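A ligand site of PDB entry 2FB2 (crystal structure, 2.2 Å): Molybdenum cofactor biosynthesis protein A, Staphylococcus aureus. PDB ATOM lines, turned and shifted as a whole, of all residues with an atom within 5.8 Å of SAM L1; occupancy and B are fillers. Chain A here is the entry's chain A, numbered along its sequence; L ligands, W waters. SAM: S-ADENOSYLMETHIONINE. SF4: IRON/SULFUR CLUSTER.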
ATOM      1  N   CYS A  24     -32.350 -11.742 -20.137  1.00  0.00           N
ATOM      2  CA  CYS A  24     -31.842 -13.060 -20.534  1.00  0.00           C
ATOM      3  C   CYS A  24     -32.809 -13.801 -21.437  1.00  0.00           C
ATOM      4  O   CYS A  24     -34.021 -13.562 -21.413  1.00  0.00           O
ATOM      5  CB  CYS A  24     -31.477 -13.886 -19.294  1.00  0.00           C
ATOM      6  SG  CYS A  24     -30.679 -15.480 -19.620  1.00  0.00           S
ATOM      7  N   TYR A  30     -32.598 -21.893 -10.990  1.00  0.00           N
ATOM      8  CA  TYR A  30     -31.774 -21.508  -9.862  1.00  0.00           C
ATOM      9  C   TYR A  30     -31.180 -20.105  -9.993  1.00  0.00           C
ATOM     10  O   TYR A  30     -30.479 -19.659  -9.092  1.00  0.00           O
ATOM     11  CB  TYR A  30     -30.689 -22.564  -9.618  1.00  0.00           C
ATOM     12  CG  TYR A  30     -29.642 -22.698 -10.710  1.00  0.00           C
ATOM     13  CD1 TYR A  30     -28.483 -21.939 -10.678  1.00  0.00           C
ATOM     14  CD2 TYR A  30     -29.787 -23.633 -11.764  1.00  0.00           C
ATOM     15  CE1 TYR A  30     -27.491 -22.046 -11.661  1.00  0.00           C
ATOM     16  CE2 TYR A  30     -28.807 -23.752 -12.764  1.00  0.00           C
ATOM     17  CZ  TYR A  30     -27.658 -22.953 -12.703  1.00  0.00           C
ATOM     18  OH  TYR A  30     -26.662 -23.037 -13.648  1.00  0.00           O
ATOM     19  N   CYS A  31     -31.490 -19.406 -11.091  1.00  0.00           N
ATOM     20  CA  CYS A  31     -30.896 -18.093 -11.398  1.00  0.00           C
ATOM     21  C   CYS A  31     -31.957 -17.038 -11.738  1.00  0.00           C
ATOM     22  O   CYS A  31     -32.070 -16.009 -11.052  1.00  0.00           O
ATOM     23  CB  CYS A  31     -29.924 -18.232 -12.568  1.00  0.00           C
ATOM     24  SG  CYS A  31     -29.216 -16.648 -13.089  1.00  0.00           S
ATOM     25  N   ARG A  71     -14.227  -9.587 -17.550  1.00  0.00           N
ATOM     26  CA  ARG A  71     -15.166 -10.659 -17.851  1.00  0.00           C
ATOM     27  C   ARG A  71     -16.534 -10.045 -18.144  1.00  0.00           C
ATOM     28  O   ARG A  71     -17.042  -9.243 -17.331  1.00  0.00           O
ATOM     29  CB  ARG A  71     -15.259 -11.578 -16.655  1.00  0.00           C
ATOM     30  CG  ARG A  71     -15.844 -12.960 -16.955  1.00  0.00           C
ATOM     31  CD  ARG A  71     -15.922 -13.749 -15.639  1.00  0.00           C
ATOM     32  NE  ARG A  71     -17.236 -14.333 -15.534  1.00  0.00           N
ATOM     33  CZ  ARG A  71     -18.155 -14.036 -14.620  1.00  0.00           C
ATOM     34  NH1 ARG A  71     -17.910 -13.180 -13.639  1.00  0.00           N
ATOM     35  NH2 ARG A  71     -19.319 -14.665 -14.681  1.00  0.00           N
ATOM     36  N   THR A  73     -20.440 -10.332 -18.692  1.00  0.00           N
ATOM     37  CA  THR A  73     -21.472 -11.207 -18.188  1.00  0.00           C
ATOM     38  C   THR A  73     -22.811 -10.462 -18.170  1.00  0.00           C
ATOM     39  O   THR A  73     -22.960  -9.390 -18.785  1.00  0.00           O
ATOM     40  CB  THR A  73     -21.052 -11.825 -16.820  1.00  0.00           C
ATOM     41  OG1 THR A  73     -22.024 -12.807 -16.410  1.00  0.00           O
ATOM     42  CG2 THR A  73     -20.921 -10.739 -15.724  1.00  0.00           C
ATOM     43  N   GLY A  74     -23.798 -11.015 -17.453  1.00  0.00           N
ATOM     44  CA  GLY A  74     -25.152 -10.476 -17.458  1.00  0.00           C
ATOM     45  C   GLY A  74     -25.910 -11.094 -16.288  1.00  0.00           C
ATOM     46  O   GLY A  74     -25.289 -11.343 -15.259  1.00  0.00           O
ATOM     47  N   GLY A  75     -27.186 -11.452 -16.462  1.00  0.00           N
ATOM     48  CA  GLY A  75     -27.849 -11.476 -17.758  1.00  0.00           C
ATOM     49  C   GLY A  75     -27.167 -12.392 -18.777  1.00  0.00           C
ATOM     50  O   GLY A  75     -26.145 -13.041 -18.492  1.00  0.00           O
ATOM     51  N   GLU A  76     -27.725 -12.435 -19.968  1.00  0.00           N
ATOM     52  CA  GLU A  76     -27.069 -13.076 -21.075  1.00  0.00           C
ATOM     53  C   GLU A  76     -26.455 -11.937 -21.902  1.00  0.00           C
ATOM     54  O   GLU A  76     -27.179 -11.178 -22.534  1.00  0.00           O
ATOM     55  CB  GLU A  76     -28.073 -13.890 -21.904  1.00  0.00           C
ATOM     56  CG  GLU A  76     -27.568 -14.253 -23.270  1.00  0.00           C
ATOM     57  CD  GLU A  76     -26.171 -14.935 -23.201  1.00  0.00           C
ATOM     58  OE1 GLU A  76     -25.374 -14.652 -24.098  1.00  0.00           O
ATOM     59  OE2 GLU A  76     -25.900 -15.740 -22.282  1.00  0.00           O
ATOM     60  N   PRO A  77     -25.130 -11.832 -21.880  1.00  0.00           N
ATOM     61  CA  PRO A  77     -24.487 -10.691 -22.550  1.00  0.00           C
ATOM     62  C   PRO A  77     -24.735 -10.529 -24.066  1.00  0.00           C
ATOM     63  O   PRO A  77     -24.757  -9.402 -24.565  1.00  0.00           O
ATOM     64  CB  PRO A  77     -22.995 -10.881 -22.250  1.00  0.00           C
ATOM     65  CG  PRO A  77     -22.855 -12.372 -21.897  1.00  0.00           C
ATOM     66  CD  PRO A  77     -24.157 -12.755 -21.250  1.00  0.00           C
ATOM     67  N   THR A 102     -18.865 -14.801 -20.608  1.00  0.00           N
ATOM     68  CA  THR A 102     -19.630 -15.907 -20.072  1.00  0.00           C
ATOM     69  C   THR A 102     -21.005 -15.847 -20.718  1.00  0.00           C
ATOM     70  O   THR A 102     -21.693 -14.854 -20.601  1.00  0.00           O
ATOM     71  CB  THR A 102     -19.751 -15.780 -18.543  1.00  0.00           C
ATOM     72  OG1 THR A 102     -18.463 -15.435 -18.044  1.00  0.00           O
ATOM     73  CG2 THR A 102     -20.162 -17.080 -17.912  1.00  0.00           C
ATOM     74  N   THR A 103     -21.411 -16.906 -21.401  1.00  0.00           N
ATOM     75  CA  THR A 103     -22.645 -16.901 -22.160  1.00  0.00           C
ATOM     76  C   THR A 103     -23.294 -18.285 -22.093  1.00  0.00           C
ATOM     77  O   THR A 103     -22.589 -19.310 -21.875  1.00  0.00           O
ATOM     78  CB  THR A 103     -22.356 -16.481 -23.629  1.00  0.00           C
ATOM     79  OG1 THR A 103     -23.552 -16.471 -24.405  1.00  0.00           O
ATOM     80  CG2 THR A 103     -21.380 -17.406 -24.292  1.00  0.00           C
ATOM     81  N   ASN A 104     -24.625 -18.327 -22.260  1.00  0.00           N
ATOM     82  CA  ASN A 104     -25.317 -19.601 -22.499  1.00  0.00           C
ATOM     83  C   ASN A 104     -25.075 -20.078 -23.932  1.00  0.00           C
ATOM     84  O   ASN A 104     -25.442 -21.196 -24.291  1.00  0.00           O
ATOM     85  CB  ASN A 104     -26.829 -19.554 -22.143  1.00  0.00           C
ATOM     86  CG  ASN A 104     -27.630 -18.545 -22.994  1.00  0.00           C
ATOM     87  OD1 ASN A 104     -27.347 -18.355 -24.179  1.00  0.00           O
ATOM     88  ND2 ASN A 104     -28.644 -17.912 -22.373  1.00  0.00           N
ATOM     89  N   ASN A 124     -16.677 -18.656 -22.292  1.00  0.00           N
ATOM     90  CA  ASN A 124     -17.024 -19.700 -21.397  1.00  0.00           C
ATOM     91  C   ASN A 124     -18.498 -19.970 -21.624  1.00  0.00           C
ATOM     92  O   ASN A 124     -19.319 -19.103 -21.381  1.00  0.00           O
ATOM     93  CB  ASN A 124     -16.768 -19.286 -19.936  1.00  0.00           C
ATOM     94  CG  ASN A 124     -15.360 -18.773 -19.706  1.00  0.00           C
ATOM     95  OD1 ASN A 124     -14.374 -19.485 -19.989  1.00  0.00           O
ATOM     96  ND2 ASN A 124     -15.244 -17.504 -19.201  1.00  0.00           N
ATOM     97  N   VAL A 125     -18.829 -21.157 -22.066  1.00  0.00           N
ATOM     98  CA  VAL A 125     -20.227 -21.467 -22.303  1.00  0.00           C
ATOM     99  C   VAL A 125     -20.795 -22.226 -21.106  1.00  0.00           C
ATOM    100  O   VAL A 125     -20.246 -23.247 -20.729  1.00  0.00           O
ATOM    101  CB  VAL A 125     -20.445 -22.264 -23.640  1.00  0.00           C
ATOM    102  CG1 VAL A 125     -21.959 -22.729 -23.794  1.00  0.00           C
ATOM    103  CG2 VAL A 125     -20.049 -21.408 -24.804  1.00  0.00           C
ATOM    104  N   SER A 126     -21.839 -21.679 -20.494  1.00  0.00           N
ATOM    105  CA  SER A 126     -22.579 -22.382 -19.453  1.00  0.00           C
ATOM    106  C   SER A 126     -23.567 -23.375 -20.068  1.00  0.00           C
ATOM    107  O   SER A 126     -24.472 -22.984 -20.803  1.00  0.00           O
ATOM    108  CB  SER A 126     -23.349 -21.395 -18.577  1.00  0.00           C
ATOM    109  OG  SER A 126     -22.464 -20.431 -18.044  1.00  0.00           O
ATOM    110  N   ASP A 128     -25.694 -26.890 -18.690  1.00  0.00           N
ATOM    111  CA  ASP A 128     -25.949 -27.682 -17.495  1.00  0.00           C
ATOM    112  C   ASP A 128     -26.400 -29.113 -17.775  1.00  0.00           C
ATOM    113  O   ASP A 128     -26.575 -29.886 -16.850  1.00  0.00           O
ATOM    114  CB  ASP A 128     -26.932 -26.968 -16.540  1.00  0.00           C
ATOM    115  CG  ASP A 128     -26.228 -25.953 -15.621  1.00  0.00           C
ATOM    116  OD1 ASP A 128     -24.988 -25.736 -15.746  1.00  0.00           O
ATOM    117  OD2 ASP A 128     -26.935 -25.362 -14.767  1.00  0.00           O
ATOM    118  N   ASN A 165     -18.799 -24.682 -18.799  1.00  0.00           N
ATOM    119  CA  ASN A 165     -18.970 -24.669 -17.354  1.00  0.00           C
ATOM    120  C   ASN A 165     -20.285 -25.376 -17.077  1.00  0.00           C
ATOM    121  O   ASN A 165     -21.276 -25.065 -17.729  1.00  0.00           O
ATOM    122  CB  ASN A 165     -19.046 -23.217 -16.850  1.00  0.00           C
ATOM    123  CG  ASN A 165     -17.720 -22.482 -16.988  1.00  0.00           C
ATOM    124  OD1 ASN A 165     -16.776 -22.776 -16.247  1.00  0.00           O
ATOM    125  ND2 ASN A 165     -17.627 -21.510 -17.924  1.00  0.00           N
ATOM    126  N   VAL A 167     -22.866 -26.527 -13.771  1.00  0.00           N
ATOM    127  CA  VAL A 167     -23.270 -26.572 -12.351  1.00  0.00           C
ATOM    128  C   VAL A 167     -24.047 -27.853 -12.065  1.00  0.00           C
ATOM    129  O   VAL A 167     -25.138 -28.070 -12.619  1.00  0.00           O
ATOM    130  CB  VAL A 167     -24.119 -25.345 -11.927  1.00  0.00           C
ATOM    131  CG1 VAL A 167     -24.553 -25.423 -10.469  1.00  0.00           C
ATOM    132  CG2 VAL A 167     -23.329 -24.090 -12.163  1.00  0.00           C
ATOM    133  N   ILE A 194     -18.980 -27.505 -11.474  1.00  0.00           N
ATOM    134  CA  ILE A 194     -19.037 -26.521 -10.418  1.00  0.00           C
ATOM    135  C   ILE A 194     -20.045 -26.980  -9.359  1.00  0.00           C
ATOM    136  O   ILE A 194     -21.153 -27.371  -9.703  1.00  0.00           O
ATOM    137  CB  ILE A 194     -19.389 -25.145 -11.000  1.00  0.00           C
ATOM    138  CG1 ILE A 194     -18.399 -24.803 -12.138  1.00  0.00           C
ATOM    139  CG2 ILE A 194     -19.432 -24.054  -9.894  1.00  0.00           C
ATOM    140  CD1 ILE A 194     -18.608 -23.442 -12.847  1.00  0.00           C
ATOM    141  N   GLU A 195     -19.641 -26.988  -8.096  1.00  0.00           N
ATOM    142  CA  GLU A 195     -20.517 -27.293  -6.980  1.00  0.00           C
ATOM    143  C   GLU A 195     -21.627 -26.254  -6.882  1.00  0.00           C
ATOM    144  O   GLU A 195     -21.383 -25.057  -7.006  1.00  0.00           O
ATOM    145  CB  GLU A 195     -19.740 -27.321  -5.659  1.00  0.00           C
ATOM    146  CG  GLU A 195     -18.836 -28.549  -5.472  1.00  0.00           C
ATOM    147  CD  GLU A 195     -17.880 -28.414  -4.277  1.00  0.00           C
ATOM    148  OE1 GLU A 195     -17.845 -27.345  -3.641  1.00  0.00           O
ATOM    149  OE2 GLU A 195     -17.166 -29.382  -3.963  1.00  0.00           O
ATOM    150  N   PHE A 196     -22.843 -26.736  -6.670  1.00  0.00           N
ATOM    151  CA  PHE A 196     -24.029 -25.901  -6.534  1.00  0.00           C
ATOM    152  C   PHE A 196     -24.016 -25.136  -5.219  1.00  0.00           C
ATOM    153  O   PHE A 196     -23.914 -25.727  -4.154  1.00  0.00           O
ATOM    154  CB  PHE A 196     -25.290 -26.780  -6.650  1.00  0.00           C
ATOM    155  CG  PHE A 196     -26.579 -26.022  -6.520  1.00  0.00           C
ATOM    156  CD1 PHE A 196     -26.919 -25.035  -7.451  1.00  0.00           C
ATOM    157  CD2 PHE A 196     -27.463 -26.301  -5.486  1.00  0.00           C
ATOM    158  CE1 PHE A 196     -28.112 -24.324  -7.344  1.00  0.00           C
ATOM    159  CE2 PHE A 196     -28.674 -25.612  -5.375  1.00  0.00           C
ATOM    160  CZ  PHE A 196     -28.996 -24.613  -6.310  1.00  0.00           C
ATOM    161  N   MET A 197     -24.143 -23.812  -5.307  1.00  0.00           N
ATOM    162  CA  MET A 197     -24.157 -22.928  -4.150  1.00  0.00           C
ATOM    163  C   MET A 197     -25.598 -22.604  -3.746  1.00  0.00           C
ATOM    164  O   MET A 197     -26.377 -22.074  -4.524  1.00  0.00           O
ATOM    165  CB  MET A 197     -23.421 -21.634  -4.481  1.00  0.00           C
ATOM    166  CG  MET A 197     -22.000 -21.884  -4.989  1.00  0.00           C
ATOM    167  SD  MET A 197     -21.083 -20.363  -5.166  1.00  0.00           S
ATOM    168  CE  MET A 197     -21.719 -19.819  -6.754  1.00  0.00           C
ATOM    169  N   ASP A 198     -25.914 -22.918  -2.505  1.00  0.00           N
ATOM    170  CA  ASP A 198     -27.262 -22.847  -1.965  1.00  0.00           C
ATOM    171  C   ASP A 198     -27.091 -22.586  -0.477  1.00  0.00           C
ATOM    172  O   ASP A 198     -26.455 -23.376   0.213  1.00  0.00           O
ATOM    173  CB  ASP A 198     -27.963 -24.193  -2.197  1.00  0.00           C
ATOM    174  CG  ASP A 198     -29.466 -24.159  -1.912  1.00  0.00           C
ATOM    175  OD1 ASP A 198     -30.082 -23.070  -1.937  1.00  0.00           O
ATOM    176  OD2 ASP A 198     -30.021 -25.256  -1.669  1.00  0.00           O
ATOM    177  N   SER A 255     -16.665 -24.650  -5.115  1.00  0.00           N
ATOM    178  CA  SER A 255     -17.293 -23.418  -4.659  1.00  0.00           C
ATOM    179  C   SER A 255     -17.801 -23.487  -3.209  1.00  0.00           C
ATOM    180  O   SER A 255     -17.793 -22.479  -2.493  1.00  0.00           O
ATOM    181  CB  SER A 255     -18.382 -22.925  -5.634  1.00  0.00           C
ATOM    182  OG  SER A 255     -19.049 -23.945  -6.364  1.00  0.00           O
HETATM  183  N   SAM L   1     -26.182 -15.808 -18.815  1.00  0.00           N
HETATM  184  CA  SAM L   1     -24.743 -16.136 -18.903  1.00  0.00           C
HETATM  185  C   SAM L   1     -24.573 -17.601 -18.536  1.00  0.00           C
HETATM  186  O   SAM L   1     -25.539 -18.233 -18.042  1.00  0.00           O
HETATM  187  OXT SAM L   1     -23.485 -18.139 -18.688  1.00  0.00           O
HETATM  188  CB  SAM L   1     -23.846 -15.293 -17.965  1.00  0.00           C
HETATM  189  CG  SAM L   1     -24.426 -14.851 -16.612  1.00  0.00           C
HETATM  190  SD  SAM L   1     -24.960 -16.156 -15.491  1.00  0.00           S
HETATM  191  CE  SAM L   1     -25.631 -15.308 -14.031  1.00  0.00           C
HETATM  192  C5' SAM L   1     -23.317 -16.611 -14.872  1.00  0.00           C
HETATM  193  C4' SAM L   1     -23.179 -17.952 -14.143  1.00  0.00           C
HETATM  194  O4' SAM L   1     -23.767 -17.889 -12.852  1.00  0.00           O
HETATM  195  C3' SAM L   1     -23.797 -19.156 -14.859  1.00  0.00           C
HETATM  196  O3' SAM L   1     -22.774 -20.017 -15.392  1.00  0.00           O
HETATM  197  C2' SAM L   1     -24.580 -19.801 -13.734  1.00  0.00           C
HETATM  198  O2' SAM L   1     -24.563 -21.207 -13.752  1.00  0.00           O
HETATM  199  C1' SAM L   1     -23.942 -19.225 -12.465  1.00  0.00           C
HETATM  200  N9  SAM L   1     -24.772 -19.437 -11.252  1.00  0.00           N
HETATM  201  C8  SAM L   1     -25.933 -18.790 -10.912  1.00  0.00           C
HETATM  202  N7  SAM L   1     -26.385 -19.320  -9.742  1.00  0.00           N
HETATM  203  C5  SAM L   1     -25.537 -20.292  -9.320  1.00  0.00           C
HETATM  204  C6  SAM L   1     -25.510 -21.145  -8.201  1.00  0.00           C
HETATM  205  N6  SAM L   1     -26.475 -21.088  -7.280  1.00  0.00           N
HETATM  206  N1  SAM L   1     -24.477 -22.052  -8.061  1.00  0.00           N
HETATM  207  C2  SAM L   1     -23.471 -22.135  -9.007  1.00  0.00           C
HETATM  208  N3  SAM L   1     -23.495 -21.280 -10.106  1.00  0.00           N
HETATM  209  C4  SAM L   1     -24.510 -20.382 -10.270  1.00  0.00           C
HETATM  210 FE1  SF4 L   2     -29.749 -16.594 -17.785  1.00  0.00          FE
HETATM  211 FE2  SF4 L   2     -29.605 -19.015 -16.985  1.00  0.00          FE
HETATM  212 FE3  SF4 L   2     -27.310 -17.396 -17.465  1.00  0.00          FE
HETATM  213 FE4  SF4 L   2     -28.981 -17.092 -15.460  1.00  0.00          FE
HETATM  214  S1  SF4 L   2     -27.821 -18.746 -15.876  1.00  0.00           S
HETATM  215  S2  SF4 L   2     -28.159 -15.575 -16.689  1.00  0.00           S
HETATM  216  S3  SF4 L   2     -30.956 -17.548 -16.256  1.00  0.00           S
HETATM  217  S4  SF4 L   2     -28.824 -18.250 -18.740  1.00  0.00           S
HETATM  218  O   HOH W   1     -21.307 -21.564 -12.296  1.00  0.00           O
HETATM  219  O   HOH W   2     -21.603 -13.987 -13.675  1.00  0.00           O
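The side-chain hydroxyl (OG) of Ser 126 sits at hydrogen-bond distance from an oxygen (OXT) of SAM L1 (2.6 Å).
A nitrogen (N) of SAM L1 sits close to the backbone carbonyl oxygen (O) of Gly 75 (2.8 Å).
The side-chain hydroxyl of Tyr 30 sits at hydrogen-bond distance from an oxygen (O2') of SAM L1, 2.8 Å away.
The backbone NH (N) of Met 197 lies within hydrogen-bond range of a nitrogen (N1) of SAM L1.
The backbone carbonyl oxygen (O) of Met 197 lies within hydrogen-bond range of a nitrogen (N6) of SAM L1.
A nitrogen (N) of SAM L1 lies close to the side-chain carboxylate (OE2) of Glu 76 (3.5 Å).
ND2 of Asn 104 sits close to S4 of SF4 L2 (3.7 Å).
The side-chain sulfur (SG) of Cys 31 binds an iron atom (FE4) of SF4 L2 (2.4 Å).
An iron atom (FE1) of SF4 L2 is bound by the side-chain sulfur (SG) of Cys 24 (2.3 Å).
O of SAM L1 is bound to FE3 of SF4 L2, at 2.0 Å.
The backbone NH of Ser 126 lies within hydrogen-bond range of the backbone carbonyl oxygen of Thr 103.
OH of Tyr 30 sits at hydrogen-bond distance from OD2 of Asp 128 (2.6 Å).
OE1 of Glu 76 lies within hydrogen-bond range of OG1 of Thr 103 (2.6 Å).
N of Thr 103 lies within hydrogen-bond range of O of Asn 124, at 3.0 Å.
The side-chain hydroxyl (OG1) of Thr 102 is in hydrogen-bond range of the guanidinium group (NE) of Arg 71, 3.0 Å away.
The side-chain carboxylate (OE2) of Glu 76 sits at hydrogen-bond distance from the backbone NH (N) of Asn 104, 2.9 Å away.
The backbone NH of Val 167 lies within hydrogen-bond range of the side-chain carboxylate of Asp 128 (3.0 Å).
Water W2 bridges NH2 of Arg 71 (2.6 Å) and OG1 of Thr 73 (3.0 Å).
Merely in contact with SAM L1: Thr 73 (3.2 Å), Thr 103 (3.4 Å), Thr 102 (3.4 Å), Val 167 (3.5 Å), Phe 196 (3.6 Å), Asn 104 (3.8 Å), Gly 74 (3.9 Å) and Cys 31 (3.9 Å).
13 residues have an atom within 4 Å of SAM L1: Tyr 30, Cys 31, Thr 73, Gly 74, Gly 75, Glu 76, Thr 102, Thr 103, Asn 104, Ser 126, Val 167, Phe 196 and Met 197.
Along chain A the residues within 4 Å of SAM L1 span positions 30 to 197.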
